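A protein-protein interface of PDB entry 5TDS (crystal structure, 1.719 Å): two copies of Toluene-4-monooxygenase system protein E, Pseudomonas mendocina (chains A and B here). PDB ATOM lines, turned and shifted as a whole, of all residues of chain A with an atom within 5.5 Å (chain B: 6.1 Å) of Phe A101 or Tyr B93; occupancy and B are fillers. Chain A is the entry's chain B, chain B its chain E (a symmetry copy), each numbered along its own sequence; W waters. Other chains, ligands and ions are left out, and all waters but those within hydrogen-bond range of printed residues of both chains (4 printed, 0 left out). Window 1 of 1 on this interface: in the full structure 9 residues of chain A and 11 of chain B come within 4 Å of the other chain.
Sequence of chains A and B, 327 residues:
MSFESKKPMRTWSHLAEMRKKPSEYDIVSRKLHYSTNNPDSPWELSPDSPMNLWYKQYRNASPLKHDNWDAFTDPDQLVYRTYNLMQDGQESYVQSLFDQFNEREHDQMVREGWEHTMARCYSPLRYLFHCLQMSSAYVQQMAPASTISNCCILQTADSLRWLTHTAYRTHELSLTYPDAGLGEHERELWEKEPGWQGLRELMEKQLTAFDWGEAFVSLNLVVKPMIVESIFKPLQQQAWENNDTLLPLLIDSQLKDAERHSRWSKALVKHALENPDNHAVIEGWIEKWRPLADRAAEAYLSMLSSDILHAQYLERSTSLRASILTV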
ATOM      1  N   SER A  92      15.918 -30.668 -20.637  1.00  0.00           N
ATOM      2  CA  SER A  92      15.575 -29.386 -21.253  1.00  0.00           C
ATOM      3  C   SER A  92      16.840 -28.620 -21.569  1.00  0.00           C
ATOM      4  O   SER A  92      16.983 -28.047 -22.648  1.00  0.00           O
ATOM      5  CB  SER A  92      14.674 -28.550 -20.344  1.00  0.00           C
ATOM      6  OG  SER A  92      13.339 -29.013 -20.428  1.00  0.00           O
ATOM      7  N   TYR A  93      17.756 -28.602 -20.609  1.00  0.00           N
ATOM      8  CA  TYR A  93      19.060 -27.992 -20.819  1.00  0.00           C
ATOM      9  C   TYR A  93      19.786 -28.631 -22.008  1.00  0.00           C
ATOM     10  O   TYR A  93      20.262 -27.935 -22.895  1.00  0.00           O
ATOM     11  CB  TYR A  93      19.891 -28.099 -19.542  1.00  0.00           C
ATOM     12  CG  TYR A  93      21.375 -27.945 -19.748  1.00  0.00           C
ATOM     13  CD1 TYR A  93      21.962 -26.688 -19.835  1.00  0.00           C
ATOM     14  CD2 TYR A  93      22.195 -29.058 -19.822  1.00  0.00           C
ATOM     15  CE1 TYR A  93      23.332 -26.547 -20.014  1.00  0.00           C
ATOM     16  CE2 TYR A  93      23.557 -28.928 -20.000  1.00  0.00           C
ATOM     17  CZ  TYR A  93      24.122 -27.679 -20.091  1.00  0.00           C
ATOM     18  OH  TYR A  93      25.481 -27.577 -20.266  1.00  0.00           O
ATOM     19  N   SER A  96      18.164 -27.802 -25.453  1.00  0.00           N
ATOM     20  CA  SER A  96      18.438 -26.444 -25.920  1.00  0.00           C
ATOM     21  C   SER A  96      19.884 -26.340 -26.365  1.00  0.00           C
ATOM     22  O   SER A  96      20.192 -25.654 -27.342  1.00  0.00           O
ATOM     23  CB  SER A  96      18.142 -25.406 -24.830  1.00  0.00           C
ATOM     24  OG  SER A  96      16.753 -25.337 -24.567  1.00  0.00           O
ATOM     25  N   LEU A  97      20.772 -27.030 -25.648  1.00  0.00           N
ATOM     26  CA  LEU A  97      22.169 -27.098 -26.042  1.00  0.00           C
ATOM     27  C   LEU A  97      22.304 -27.643 -27.467  1.00  0.00           C
ATOM     28  O   LEU A  97      22.912 -27.011 -28.340  1.00  0.00           O
ATOM     29  CB  LEU A  97      22.943 -27.984 -25.061  1.00  0.00           C
ATOM     30  CG  LEU A  97      24.460 -27.949 -25.065  1.00  0.00           C
ATOM     31  CD1 LEU A  97      24.994 -26.609 -24.559  1.00  0.00           C
ATOM     32  CD2 LEU A  97      24.947 -29.081 -24.182  1.00  0.00           C
ATOM     33  N   PHE A  98      21.730 -28.818 -27.701  1.00  0.00           N
ATOM     34  CA  PHE A  98      21.795 -29.452 -29.020  1.00  0.00           C
ATOM     35  C   PHE A  98      21.166 -28.562 -30.093  1.00  0.00           C
ATOM     36  O   PHE A  98      21.763 -28.327 -31.139  1.00  0.00           O
ATOM     37  CB  PHE A  98      21.087 -30.814 -29.021  1.00  0.00           C
ATOM     38  CG  PHE A  98      21.805 -31.892 -28.242  1.00  0.00           C
ATOM     39  CD1 PHE A  98      23.100 -31.709 -27.785  1.00  0.00           C
ATOM     40  CD2 PHE A  98      21.179 -33.109 -27.989  1.00  0.00           C
ATOM     41  CE1 PHE A  98      23.753 -32.716 -27.062  1.00  0.00           C
ATOM     42  CE2 PHE A  98      21.828 -34.122 -27.272  1.00  0.00           C
ATOM     43  CZ  PHE A  98      23.115 -33.924 -26.817  1.00  0.00           C
ATOM     44  N   ASP A  99      19.958 -28.072 -29.826  1.00  0.00           N
ATOM     45  CA  ASP A  99      19.208 -27.285 -30.812  1.00  0.00           C
ATOM     46  C   ASP A  99      19.962 -26.013 -31.204  1.00  0.00           C
ATOM     47  O   ASP A  99      20.183 -25.738 -32.393  1.00  0.00           O
ATOM     48  CB  ASP A  99      17.825 -26.927 -30.249  1.00  0.00           C
ATOM     49  CG  ASP A  99      16.827 -26.500 -31.325  1.00  0.00           C
ATOM     50  OD1 ASP A  99      17.201 -26.329 -32.500  1.00  0.00           O
ATOM     51  OD2 ASP A  99      15.639 -26.336 -30.983  1.00  0.00           O
ATOM     52  N   GLN A 100      20.365 -25.232 -30.205  1.00  0.00           N
ATOM     53  CA  GLN A 100      20.980 -23.938 -30.493  1.00  0.00           C
ATOM     54  C   GLN A 100      22.401 -24.088 -31.038  1.00  0.00           C
ATOM     55  O   GLN A 100      22.822 -23.319 -31.908  1.00  0.00           O
ATOM     56  CB  GLN A 100      20.947 -23.054 -29.243  1.00  0.00           C
ATOM     57  CG  GLN A 100      19.501 -22.712 -28.869  1.00  0.00           C
ATOM     58  CD  GLN A 100      19.363 -21.821 -27.652  1.00  0.00           C
ATOM     59  OE1 GLN A 100      20.206 -20.961 -27.392  1.00  0.00           O
ATOM     60  NE2 GLN A 100      18.279 -22.012 -26.903  1.00  0.00           N
ATOM     61  N   PHE A 101      23.147 -25.074 -30.558  1.00  0.00           N
ATOM     62  CA  PHE A 101      24.491 -25.281 -31.112  1.00  0.00           C
ATOM     63  C   PHE A 101      24.406 -25.752 -32.563  1.00  0.00           C
ATOM     64  O   PHE A 101      25.247 -25.400 -33.397  1.00  0.00           O
ATOM     65  CB  PHE A 101      25.281 -26.279 -30.269  1.00  0.00           C
ATOM     66  CG  PHE A 101      25.939 -25.662 -29.070  1.00  0.00           C
ATOM     67  CD1 PHE A 101      25.201 -24.900 -28.177  1.00  0.00           C
ATOM     68  CD2 PHE A 101      27.284 -25.832 -28.843  1.00  0.00           C
ATOM     69  CE1 PHE A 101      25.795 -24.339 -27.064  1.00  0.00           C
ATOM     70  CE2 PHE A 101      27.887 -25.270 -27.737  1.00  0.00           C
ATOM     71  CZ  PHE A 101      27.141 -24.524 -26.842  1.00  0.00           C
ATOM     72  N   ASN A 102      23.395 -26.553 -32.868  1.00  0.00           N
ATOM     73  CA  ASN A 102      23.180 -26.977 -34.247  1.00  0.00           C
ATOM     74  C   ASN A 102      22.836 -25.788 -35.143  1.00  0.00           C
ATOM     75  O   ASN A 102      23.323 -25.682 -36.270  1.00  0.00           O
ATOM     76  CB  ASN A 102      22.076 -28.035 -34.315  1.00  0.00           C
ATOM     77  CG  ASN A 102      21.668 -28.352 -35.730  1.00  0.00           C
ATOM     78  OD1 ASN A 102      22.212 -29.257 -36.366  1.00  0.00           O
ATOM     79  ND2 ASN A 102      20.714 -27.594 -36.241  1.00  0.00           N
ATOM     80  N   GLU A 103      22.004 -24.885 -34.636  1.00  0.00           N
ATOM     81  CA  GLU A 103      21.605 -23.716 -35.418  1.00  0.00           C
ATOM     82  C   GLU A 103      22.794 -22.856 -35.819  1.00  0.00           C
ATOM     83  O   GLU A 103      22.800 -22.255 -36.897  1.00  0.00           O
ATOM     84  CB  GLU A 103      20.599 -22.866 -34.647  1.00  0.00           C
ATOM     85  CG  GLU A 103      19.200 -23.460 -34.622  1.00  0.00           C
ATOM     86  CD  GLU A 103      18.605 -23.582 -36.009  1.00  0.00           C
ATOM     87  OE1 GLU A 103      17.994 -24.628 -36.308  1.00  0.00           O
ATOM     88  OE2 GLU A 103      18.751 -22.625 -36.801  1.00  0.00           O
ATOM     89  N   ARG A 104      23.800 -22.783 -34.954  1.00  0.00           N
ATOM     90  CA  ARG A 104      24.953 -21.943 -35.278  1.00  0.00           C
ATOM     91  C   ARG A 104      26.094 -22.761 -35.880  1.00  0.00           C
ATOM     92  O   ARG A 104      27.221 -22.278 -36.007  1.00  0.00           O
ATOM     93  CB  ARG A 104      25.425 -21.159 -34.057  1.00  0.00           C
ATOM     94  CG  ARG A 104      26.009 -21.968 -32.924  1.00  0.00           C
ATOM     95  CD  ARG A 104      26.474 -21.018 -31.816  1.00  0.00           C
ATOM     96  NE  ARG A 104      26.897 -21.710 -30.599  1.00  0.00           N
ATOM     97  CZ  ARG A 104      28.109 -22.230 -30.411  1.00  0.00           C
ATOM     98  NH1 ARG A 104      28.399 -22.826 -29.269  1.00  0.00           N
ATOM     99  NH2 ARG A 104      29.035 -22.154 -31.360  1.00  0.00           N
ATOM    100  N   GLU A 105      25.777 -23.988 -36.284  1.00  0.00           N
ATOM    101  CA  GLU A 105      26.725 -24.845 -36.993  1.00  0.00           C
ATOM    102  C   GLU A 105      28.016 -25.049 -36.199  1.00  0.00           C
ATOM    103  O   GLU A 105      29.116 -25.020 -36.752  1.00  0.00           O
ATOM    104  CB  GLU A 105      27.019 -24.259 -38.372  1.00  0.00           C
ATOM    105  CG  GLU A 105      25.784 -24.207 -39.255  1.00  0.00           C
ATOM    106  CD  GLU A 105      25.993 -23.419 -40.535  1.00  0.00           C
ATOM    107  OE1 GLU A 105      26.832 -22.490 -40.545  1.00  0.00           O
ATOM    108  OE2 GLU A 105      25.314 -23.731 -41.534  1.00  0.00           O
ATOM    109  N   HIS A 106      27.862 -25.247 -34.893  1.00  0.00           N
ATOM    110  CA  HIS A 106      28.986 -25.550 -34.009  1.00  0.00           C
ATOM    111  C   HIS A 106      29.967 -26.592 -34.567  1.00  0.00           C
ATOM    112  O   HIS A 106      31.183 -26.412 -34.506  1.00  0.00           O
ATOM    113  CB  HIS A 106      28.459 -26.035 -32.649  1.00  0.00           C
ATOM    114  CG  HIS A 106      29.503 -26.700 -31.801  1.00  0.00           C
ATOM    115  ND1 HIS A 106      29.852 -28.025 -31.954  1.00  0.00           N
ATOM    116  CD2 HIS A 106      30.280 -26.219 -30.802  1.00  0.00           C
ATOM    117  CE1 HIS A 106      30.801 -28.332 -31.086  1.00  0.00           C
ATOM    118  NE2 HIS A 106      31.085 -27.251 -30.381  1.00  0.00           N
ATOM    119  N   ASP A 107      29.455 -27.692 -35.099  1.00  0.00           N
ATOM    120  CA  ASP A 107      30.348 -28.786 -35.465  1.00  0.00           C
ATOM    121  C   ASP A 107      31.307 -28.410 -36.598  1.00  0.00           C
ATOM    122  O   ASP A 107      32.396 -28.965 -36.701  1.00  0.00           O
ATOM    123  CB  ASP A 107      29.544 -30.024 -35.839  1.00  0.00           C
ATOM    124  CG  ASP A 107      28.800 -30.611 -34.649  1.00  0.00           C
ATOM    125  OD1 ASP A 107      29.151 -30.275 -33.490  1.00  0.00           O
ATOM    126  OD2 ASP A 107      27.869 -31.408 -34.875  1.00  0.00           O
ATOM    127  N   THR A 245      32.927 -26.618 -28.033  1.00  0.00           N
ATOM    128  CA  THR A 245      32.320 -26.048 -26.840  1.00  0.00           C
ATOM    129  C   THR A 245      31.081 -26.829 -26.397  1.00  0.00           C
ATOM    130  O   THR A 245      30.587 -26.631 -25.288  1.00  0.00           O
ATOM    131  CB  THR A 245      31.935 -24.568 -27.045  1.00  0.00           C
ATOM    132  OG1 THR A 245      31.140 -24.426 -28.227  1.00  0.00           O
ATOM    133  CG2 THR A 245      33.178 -23.729 -27.198  1.00  0.00           C
ATOM    134  N   LEU A 246      30.583 -27.707 -27.261  1.00  0.00           N
ATOM    135  CA  LEU A 246      29.398 -28.504 -26.938  1.00  0.00           C
ATOM    136  C   LEU A 246      29.727 -29.638 -25.972  1.00  0.00           C
ATOM    137  O   LEU A 246      29.065 -29.813 -24.944  1.00  0.00           O
ATOM    138  CB  LEU A 246      28.771 -29.072 -28.215  1.00  0.00           C
ATOM    139  CG  LEU A 246      27.436 -29.804 -28.082  1.00  0.00           C
ATOM    140  CD1 LEU A 246      26.567 -29.079 -27.101  1.00  0.00           C
ATOM    141  CD2 LEU A 246      26.744 -29.903 -29.445  1.00  0.00           C
ATOM    142  N   LEU A 249      30.032 -28.988 -22.215  1.00  0.00           N
ATOM    143  CA  LEU A 249      28.770 -28.581 -21.592  1.00  0.00           C
ATOM    144  C   LEU A 249      27.832 -29.769 -21.453  1.00  0.00           C
ATOM    145  O   LEU A 249      27.032 -29.842 -20.507  1.00  0.00           O
ATOM    146  CB  LEU A 249      28.105 -27.470 -22.407  1.00  0.00           C
ATOM    147  CG  LEU A 249      28.848 -26.135 -22.361  1.00  0.00           C
ATOM    148  CD1 LEU A 249      28.168 -25.120 -23.262  1.00  0.00           C
ATOM    149  CD2 LEU A 249      28.897 -25.615 -20.945  1.00  0.00           C
ATOM    150  N   ASP B  88      10.193 -21.790 -19.088  1.00  0.00           N
ATOM    151  CA  ASP B  88      10.803 -22.484 -17.959  1.00  0.00           C
ATOM    152  C   ASP B  88      11.938 -23.375 -18.475  1.00  0.00           C
ATOM    153  O   ASP B  88      12.992 -23.513 -17.835  1.00  0.00           O
ATOM    154  CB  ASP B  88       9.782 -23.323 -17.194  1.00  0.00           C
ATOM    155  CG  ASP B  88      10.410 -24.051 -16.027  1.00  0.00           C
ATOM    156  OD1 ASP B  88      11.126 -23.409 -15.230  1.00  0.00           O
ATOM    157  OD2 ASP B  88      10.219 -25.270 -15.917  1.00  0.00           O
ATOM    158  N   GLY B  89      11.730 -23.953 -19.655  1.00  0.00           N
ATOM    159  CA  GLY B  89      12.765 -24.731 -20.310  1.00  0.00           C
ATOM    160  C   GLY B  89      13.968 -23.879 -20.679  1.00  0.00           C
ATOM    161  O   GLY B  89      15.110 -24.275 -20.430  1.00  0.00           O
ATOM    162  N   GLN B  90      13.725 -22.709 -21.265  1.00  0.00           N
ATOM    163  CA  GLN B  90      14.830 -21.838 -21.667  1.00  0.00           C
ATOM    164  C   GLN B  90      15.579 -21.330 -20.450  1.00  0.00           C
ATOM    165  O   GLN B  90      16.798 -21.174 -20.487  1.00  0.00           O
ATOM    166  CB  GLN B  90      14.345 -20.636 -22.486  1.00  0.00           C
ATOM    167  CG  GLN B  90      14.120 -20.901 -23.951  1.00  0.00           C
ATOM    168  CD  GLN B  90      15.333 -21.439 -24.659  1.00  0.00           C
ATOM    169  OE1 GLN B  90      16.387 -20.782 -24.747  1.00  0.00           O
ATOM    170  NE2 GLN B  90      15.198 -22.643 -25.183  1.00  0.00           N
ATOM    171  N   GLU B  91      14.860 -21.049 -19.369  1.00  0.00           N
ATOM    172  CA  GLU B  91      15.539 -20.578 -18.163  1.00  0.00           C
ATOM    173  C   GLU B  91      16.303 -21.709 -17.474  1.00  0.00           C
ATOM    174  O   GLU B  91      17.347 -21.464 -16.880  1.00  0.00           O
ATOM    175  CB  GLU B  91      14.552 -19.927 -17.187  1.00  0.00           C
ATOM    176  CG  GLU B  91      14.136 -18.506 -17.577  1.00  0.00           C
ATOM    177  CD  GLU B  91      15.312 -17.515 -17.628  1.00  0.00           C
ATOM    178  OE1 GLU B  91      15.952 -17.378 -18.693  1.00  0.00           O
ATOM    179  OE2 GLU B  91      15.590 -16.852 -16.608  1.00  0.00           O
ATOM    180  N   SER B  92      15.806 -22.941 -17.555  1.00  0.00           N
ATOM    181  CA  SER B  92      16.586 -24.082 -17.070  1.00  0.00           C
ATOM    182  C   SER B  92      17.912 -24.166 -17.818  1.00  0.00           C
ATOM    183  O   SER B  92      18.955 -24.453 -17.229  1.00  0.00           O
ATOM    184  CB  SER B  92      15.817 -25.395 -17.228  1.00  0.00           C
ATOM    185  OG  SER B  92      14.694 -25.413 -16.373  1.00  0.00           O
ATOM    186  N   TYR B  93      17.860 -23.921 -19.121  1.00  0.00           N
ATOM    187  CA  TYR B  93      19.064 -23.907 -19.945  1.00  0.00           C
ATOM    188  C   TYR B  93      20.029 -22.813 -19.468  1.00  0.00           C
ATOM    189  O   TYR B  93      21.173 -23.087 -19.108  1.00  0.00           O
ATOM    190  CB  TYR B  93      18.677 -23.711 -21.423  1.00  0.00           C
ATOM    191  CG  TYR B  93      19.831 -23.517 -22.374  1.00  0.00           C
ATOM    192  CD1 TYR B  93      20.809 -24.489 -22.519  1.00  0.00           C
ATOM    193  CD2 TYR B  93      19.929 -22.367 -23.145  1.00  0.00           C
ATOM    194  CE1 TYR B  93      21.862 -24.322 -23.391  1.00  0.00           C
ATOM    195  CE2 TYR B  93      20.987 -22.184 -24.028  1.00  0.00           C
ATOM    196  CZ  TYR B  93      21.949 -23.167 -24.143  1.00  0.00           C
ATOM    197  OH  TYR B  93      22.996 -23.015 -25.014  1.00  0.00           O
ATOM    198  N   VAL B  94      19.561 -21.568 -19.439  1.00  0.00           N
ATOM    199  CA  VAL B  94      20.430 -20.458 -19.070  1.00  0.00           C
ATOM    200  C   VAL B  94      20.944 -20.568 -17.630  1.00  0.00           C
ATOM    201  O   VAL B  94      22.120 -20.333 -17.377  1.00  0.00           O
ATOM    202  CB  VAL B  94      19.710 -19.112 -19.255  1.00  0.00           C
ATOM    203  CG1 VAL B  94      20.530 -17.990 -18.657  1.00  0.00           C
ATOM    204  CG2 VAL B  94      19.461 -18.857 -20.739  1.00  0.00           C
ATOM    205  N   GLN B  95      20.079 -20.936 -16.686  1.00  0.00           N
ATOM    206  CA  GLN B  95      20.514 -20.969 -15.297  1.00  0.00           C
ATOM    207  C   GLN B  95      21.563 -22.072 -15.109  1.00  0.00           C
ATOM    208  O   GLN B  95      22.482 -21.939 -14.296  1.00  0.00           O
ATOM    209  CB  GLN B  95      19.322 -21.158 -14.350  1.00  0.00           C
ATOM    210  CG  GLN B  95      18.177 -20.123 -14.544  1.00  0.00           C
ATOM    211  CD  GLN B  95      18.594 -18.651 -14.368  1.00  0.00           C
ATOM    212  OE1 GLN B  95      18.355 -17.803 -15.248  1.00  0.00           O
ATOM    213  NE2 GLN B  95      19.174 -18.337 -13.218  1.00  0.00           N
ATOM    214  N   SER B  96      21.453 -23.142 -15.889  1.00  0.00           N
ATOM    215  CA  SER B  96      22.453 -24.202 -15.839  1.00  0.00           C
ATOM    216  C   SER B  96      23.773 -23.700 -16.414  1.00  0.00           C
ATOM    217  O   SER B  96      24.838 -23.994 -15.874  1.00  0.00           O
ATOM    218  CB  SER B  96      21.983 -25.444 -16.591  1.00  0.00           C
ATOM    219  OG  SER B  96      20.838 -25.995 -15.959  1.00  0.00           O
ATOM    220  N   LEU B  97      23.712 -22.933 -17.500  1.00  0.00           N
ATOM    221  CA  LEU B  97      24.947 -22.369 -18.050  1.00  0.00           C
ATOM    222  C   LEU B  97      25.636 -21.462 -17.037  1.00  0.00           C
ATOM    223  O   LEU B  97      26.846 -21.551 -16.852  1.00  0.00           O
ATOM    224  CB  LEU B  97      24.683 -21.582 -19.341  1.00  0.00           C
ATOM    225  CG  LEU B  97      24.196 -22.382 -20.548  1.00  0.00           C
ATOM    226  CD1 LEU B  97      23.805 -21.430 -21.670  1.00  0.00           C
ATOM    227  CD2 LEU B  97      25.269 -23.367 -21.010  1.00  0.00           C
ATOM    228  N   PHE B  98      24.873 -20.581 -16.394  1.00  0.00           N
ATOM    229  CA  PHE B  98      25.444 -19.666 -15.405  1.00  0.00           C
ATOM    230  C   PHE B  98      26.181 -20.463 -14.334  1.00  0.00           C
ATOM    231  O   PHE B  98      27.322 -20.160 -13.986  1.00  0.00           O
ATOM    232  CB  PHE B  98      24.361 -18.805 -14.735  1.00  0.00           C
ATOM    233  CG  PHE B  98      23.810 -17.705 -15.603  1.00  0.00           C
ATOM    234  CD1 PHE B  98      24.418 -17.358 -16.805  1.00  0.00           C
ATOM    235  CD2 PHE B  98      22.679 -16.999 -15.200  1.00  0.00           C
ATOM    236  CE1 PHE B  98      23.893 -16.332 -17.595  1.00  0.00           C
ATOM    237  CE2 PHE B  98      22.156 -15.971 -15.987  1.00  0.00           C
ATOM    238  CZ  PHE B  98      22.769 -15.637 -17.177  1.00  0.00           C
ATOM    239  N   TRP B 240      33.204 -14.042 -28.617  1.00  0.00           N
ATOM    240  CA  TRP B 240      33.987 -15.209 -29.017  1.00  0.00           C
ATOM    241  C   TRP B 240      35.451 -14.821 -29.221  1.00  0.00           C
ATOM    242  O   TRP B 240      36.369 -15.539 -28.811  1.00  0.00           O
ATOM    243  CB  TRP B 240      33.457 -15.831 -30.318  1.00  0.00           C
ATOM    244  CG  TRP B 240      32.161 -16.594 -30.236  1.00  0.00           C
ATOM    245  CD1 TRP B 240      30.994 -16.296 -30.895  1.00  0.00           C
ATOM    246  CD2 TRP B 240      31.906 -17.798 -29.497  1.00  0.00           C
ATOM    247  NE1 TRP B 240      30.033 -17.229 -30.596  1.00  0.00           N
ATOM    248  CE2 TRP B 240      30.564 -18.161 -29.740  1.00  0.00           C
ATOM    249  CE3 TRP B 240      32.679 -18.599 -28.648  1.00  0.00           C
ATOM    250  CZ2 TRP B 240      29.974 -19.290 -29.162  1.00  0.00           C
ATOM    251  CZ3 TRP B 240      32.091 -19.727 -28.074  1.00  0.00           C
ATOM    252  CH2 TRP B 240      30.752 -20.059 -28.335  1.00  0.00           C
ATOM    253  N   LEU B 249      26.307 -17.702 -25.903  1.00  0.00           N
ATOM    254  CA  LEU B 249      25.273 -18.707 -25.662  1.00  0.00           C
ATOM    255  C   LEU B 249      24.059 -18.069 -25.032  1.00  0.00           C
ATOM    256  O   LEU B 249      22.924 -18.414 -25.369  1.00  0.00           O
ATOM    257  CB  LEU B 249      25.788 -19.830 -24.753  1.00  0.00           C
ATOM    258  CG  LEU B 249      27.068 -20.506 -25.211  1.00  0.00           C
ATOM    259  CD1 LEU B 249      27.364 -21.688 -24.293  1.00  0.00           C
ATOM    260  CD2 LEU B 249      26.979 -20.942 -26.650  1.00  0.00           C
ATOM    261  N   LEU B 250      24.301 -17.150 -24.098  1.00  0.00           N
ATOM    262  CA  LEU B 250      23.223 -16.384 -23.479  1.00  0.00           C
ATOM    263  C   LEU B 250      22.457 -15.587 -24.531  1.00  0.00           C
ATOM    264  O   LEU B 250      21.215 -15.586 -24.564  1.00  0.00           O
ATOM    265  CB  LEU B 250      23.783 -15.438 -22.417  1.00  0.00           C
ATOM    266  CG  LEU B 250      22.804 -14.442 -21.788  1.00  0.00           C
ATOM    267  CD1 LEU B 250      21.666 -15.178 -21.087  1.00  0.00           C
ATOM    268  CD2 LEU B 250      23.547 -13.548 -20.802  1.00  0.00           C
ATOM    269  N   ASP B 252      22.216 -16.179 -27.692  1.00  0.00           N
ATOM    270  CA  ASP B 252      21.418 -17.038 -28.576  1.00  0.00           C
ATOM    271  C   ASP B 252      20.057 -17.379 -27.951  1.00  0.00           C
ATOM    272  O   ASP B 252      19.054 -17.466 -28.656  1.00  0.00           O
ATOM    273  CB  ASP B 252      22.165 -18.316 -28.931  1.00  0.00           C
ATOM    274  CG  ASP B 252      22.923 -18.214 -30.260  1.00  0.00           C
ATOM    275  OD1 ASP B 252      22.798 -17.188 -30.969  1.00  0.00           O
ATOM    276  OD2 ASP B 252      23.634 -19.185 -30.608  1.00  0.00           O
ATOM    277  N   SER B 253      20.012 -17.571 -26.638  1.00  0.00           N
ATOM    278  CA  SER B 253      18.731 -17.824 -25.986  1.00  0.00           C
ATOM    279  C   SER B 253      17.840 -16.581 -26.089  1.00  0.00           C
ATOM    280  O   SER B 253      16.640 -16.675 -26.346  1.00  0.00           O
ATOM    281  CB  SER B 253      18.927 -18.224 -24.515  1.00  0.00           C
ATOM    282  OG  SER B 253      17.671 -18.433 -23.880  1.00  0.00           O
HETATM  283  O   HOH W   1      24.482 -21.194 -29.150  1.00  0.00           O
HETATM  284  O   HOH W   2      16.034 -24.057 -27.695  1.00  0.00           O
HETATM  285  O   HOH W   3      22.755 -20.942 -26.709  1.00  0.00           O
HETATM  286  O   HOH W   4      22.181 -20.703 -32.159  1.00  0.00           O
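N of Ser B253 sits at hydrogen-bond distance from OE1 of Gln A100.
The side-chain amide nitrogen (NE2) of Gln A100 lies within hydrogen-bond range of the side-chain amide oxygen (OE1) of Gln B90 (3.1 Å).
NE2 of Gln B90 is in hydrogen-bond range of OG of Ser A96 (3.2 Å).
The backbone carbonyl oxygen (O) of Phe A101 lies within hydrogen-bond range of the backbone NH (N) of His A106 (3.0 Å).
NH1 of Arg A104 is in hydrogen-bond range of OG1 of Thr A245.
OG of Ser B253 is in hydrogen-bond range of OE1 of Gln B90, 2.8 Å away.
O of Ser A92 is in hydrogen-bond range of OG of Ser A96.
OH of Tyr A93 sits at hydrogen-bond distance from O of Leu A249 (2.8 Å).
The backbone carbonyl oxygen of Ser B92 lies within hydrogen-bond range of the side-chain hydroxyl of Ser B96 (2.7 Å).
O of Tyr A93 touches CD1 of Tyr B93, 3.5 Å away.
Ser B96 touches Tyr A93.
CD2 of Leu B97 touches CE1 of Tyr A93, at 3.9 Å.
Ser A96 touches Tyr B93.
Leu A97 touches Tyr B93.
Gln A100 touches Asp B252.
Phe A101 touches Tyr B93.
Trp B240 touches Arg A104.
OD2 of Asp B252 touches CD of Arg A104, 3.6 Å away.
CD1 of Leu A249 touches CD1 of Leu B249, at 3.7 Å.
Of chain B, only Tyr B93 (3.7 Å) and Leu B249 (3.6 Å) come within 4 Å of Phe A101.
Tyr B93 touches just these residues of chain A: Tyr A93 (3.5 Å), Ser A96 (3.5 Å), Leu A97 (3.7 Å), Gln A100 (3.7 Å) and Phe A101 (3.7 Å).
Of the printed residues of chain A, Gln B90 touches Ser A96 (3.2 Å) and Gln A100 (3.1 Å).
Of the printed residues of chain A, Trp B240 touches Arg A104 (3.7 Å).
Of the printed residues of chain B, Leu A97 touches Tyr B93.
Gln B95 touches none of the printed residues of chain A.
The nearest printed residue of chain B that does not touch Phe A101 is Asp B252 (5.9 Å).
Of the 17 printed residues of chain A, 7 touch a printed residue of chain B.
Hydrophobic or aromatic side chains of chain A that line the printed part of chain B: Tyr A93, Phe A101 and Leu A249.
Among the printed residues, no Asp or Glu carboxylate lies within 4 Å of a Lys or Arg side-chain nitrogen of the other chain.
Tyr B93 touches its own counterpart, Tyr A93.
Tyr A93 touches Ser B96, and with the chains exchanged Ser A96 touches Tyr B93.
Tyr A93 touches Leu B97, and with the chains exchanged Leu A97 touches Tyr B93.
Leu B249 touches its own counterpart, Leu A249.
Of the 16 pairs that touch across the chains among the printed residues, 6 have their exchanged pair printed and touching as well.
Water W4 lies within hydrogen-bond range of OD2 of Asp B252 and O of Gln A100.
Water W1 bridges the side-chain carboxylate (OD2) of Asp B252 (2.6 Å) and the guanidinium group (NE) of Arg A104 (2.9 Å).
Water W3 lies within hydrogen-bond range of OE1 of Gln A100, OH of Tyr B93 and O of Leu B249.
Water W2 lies within hydrogen-bond range of the side-chain amide nitrogen of Gln B90 (3.0 Å), the side-chain amide nitrogen of Gln A100 (3.1 Å) and the side-chain hydroxyl of Ser A96 (3.5 Å).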
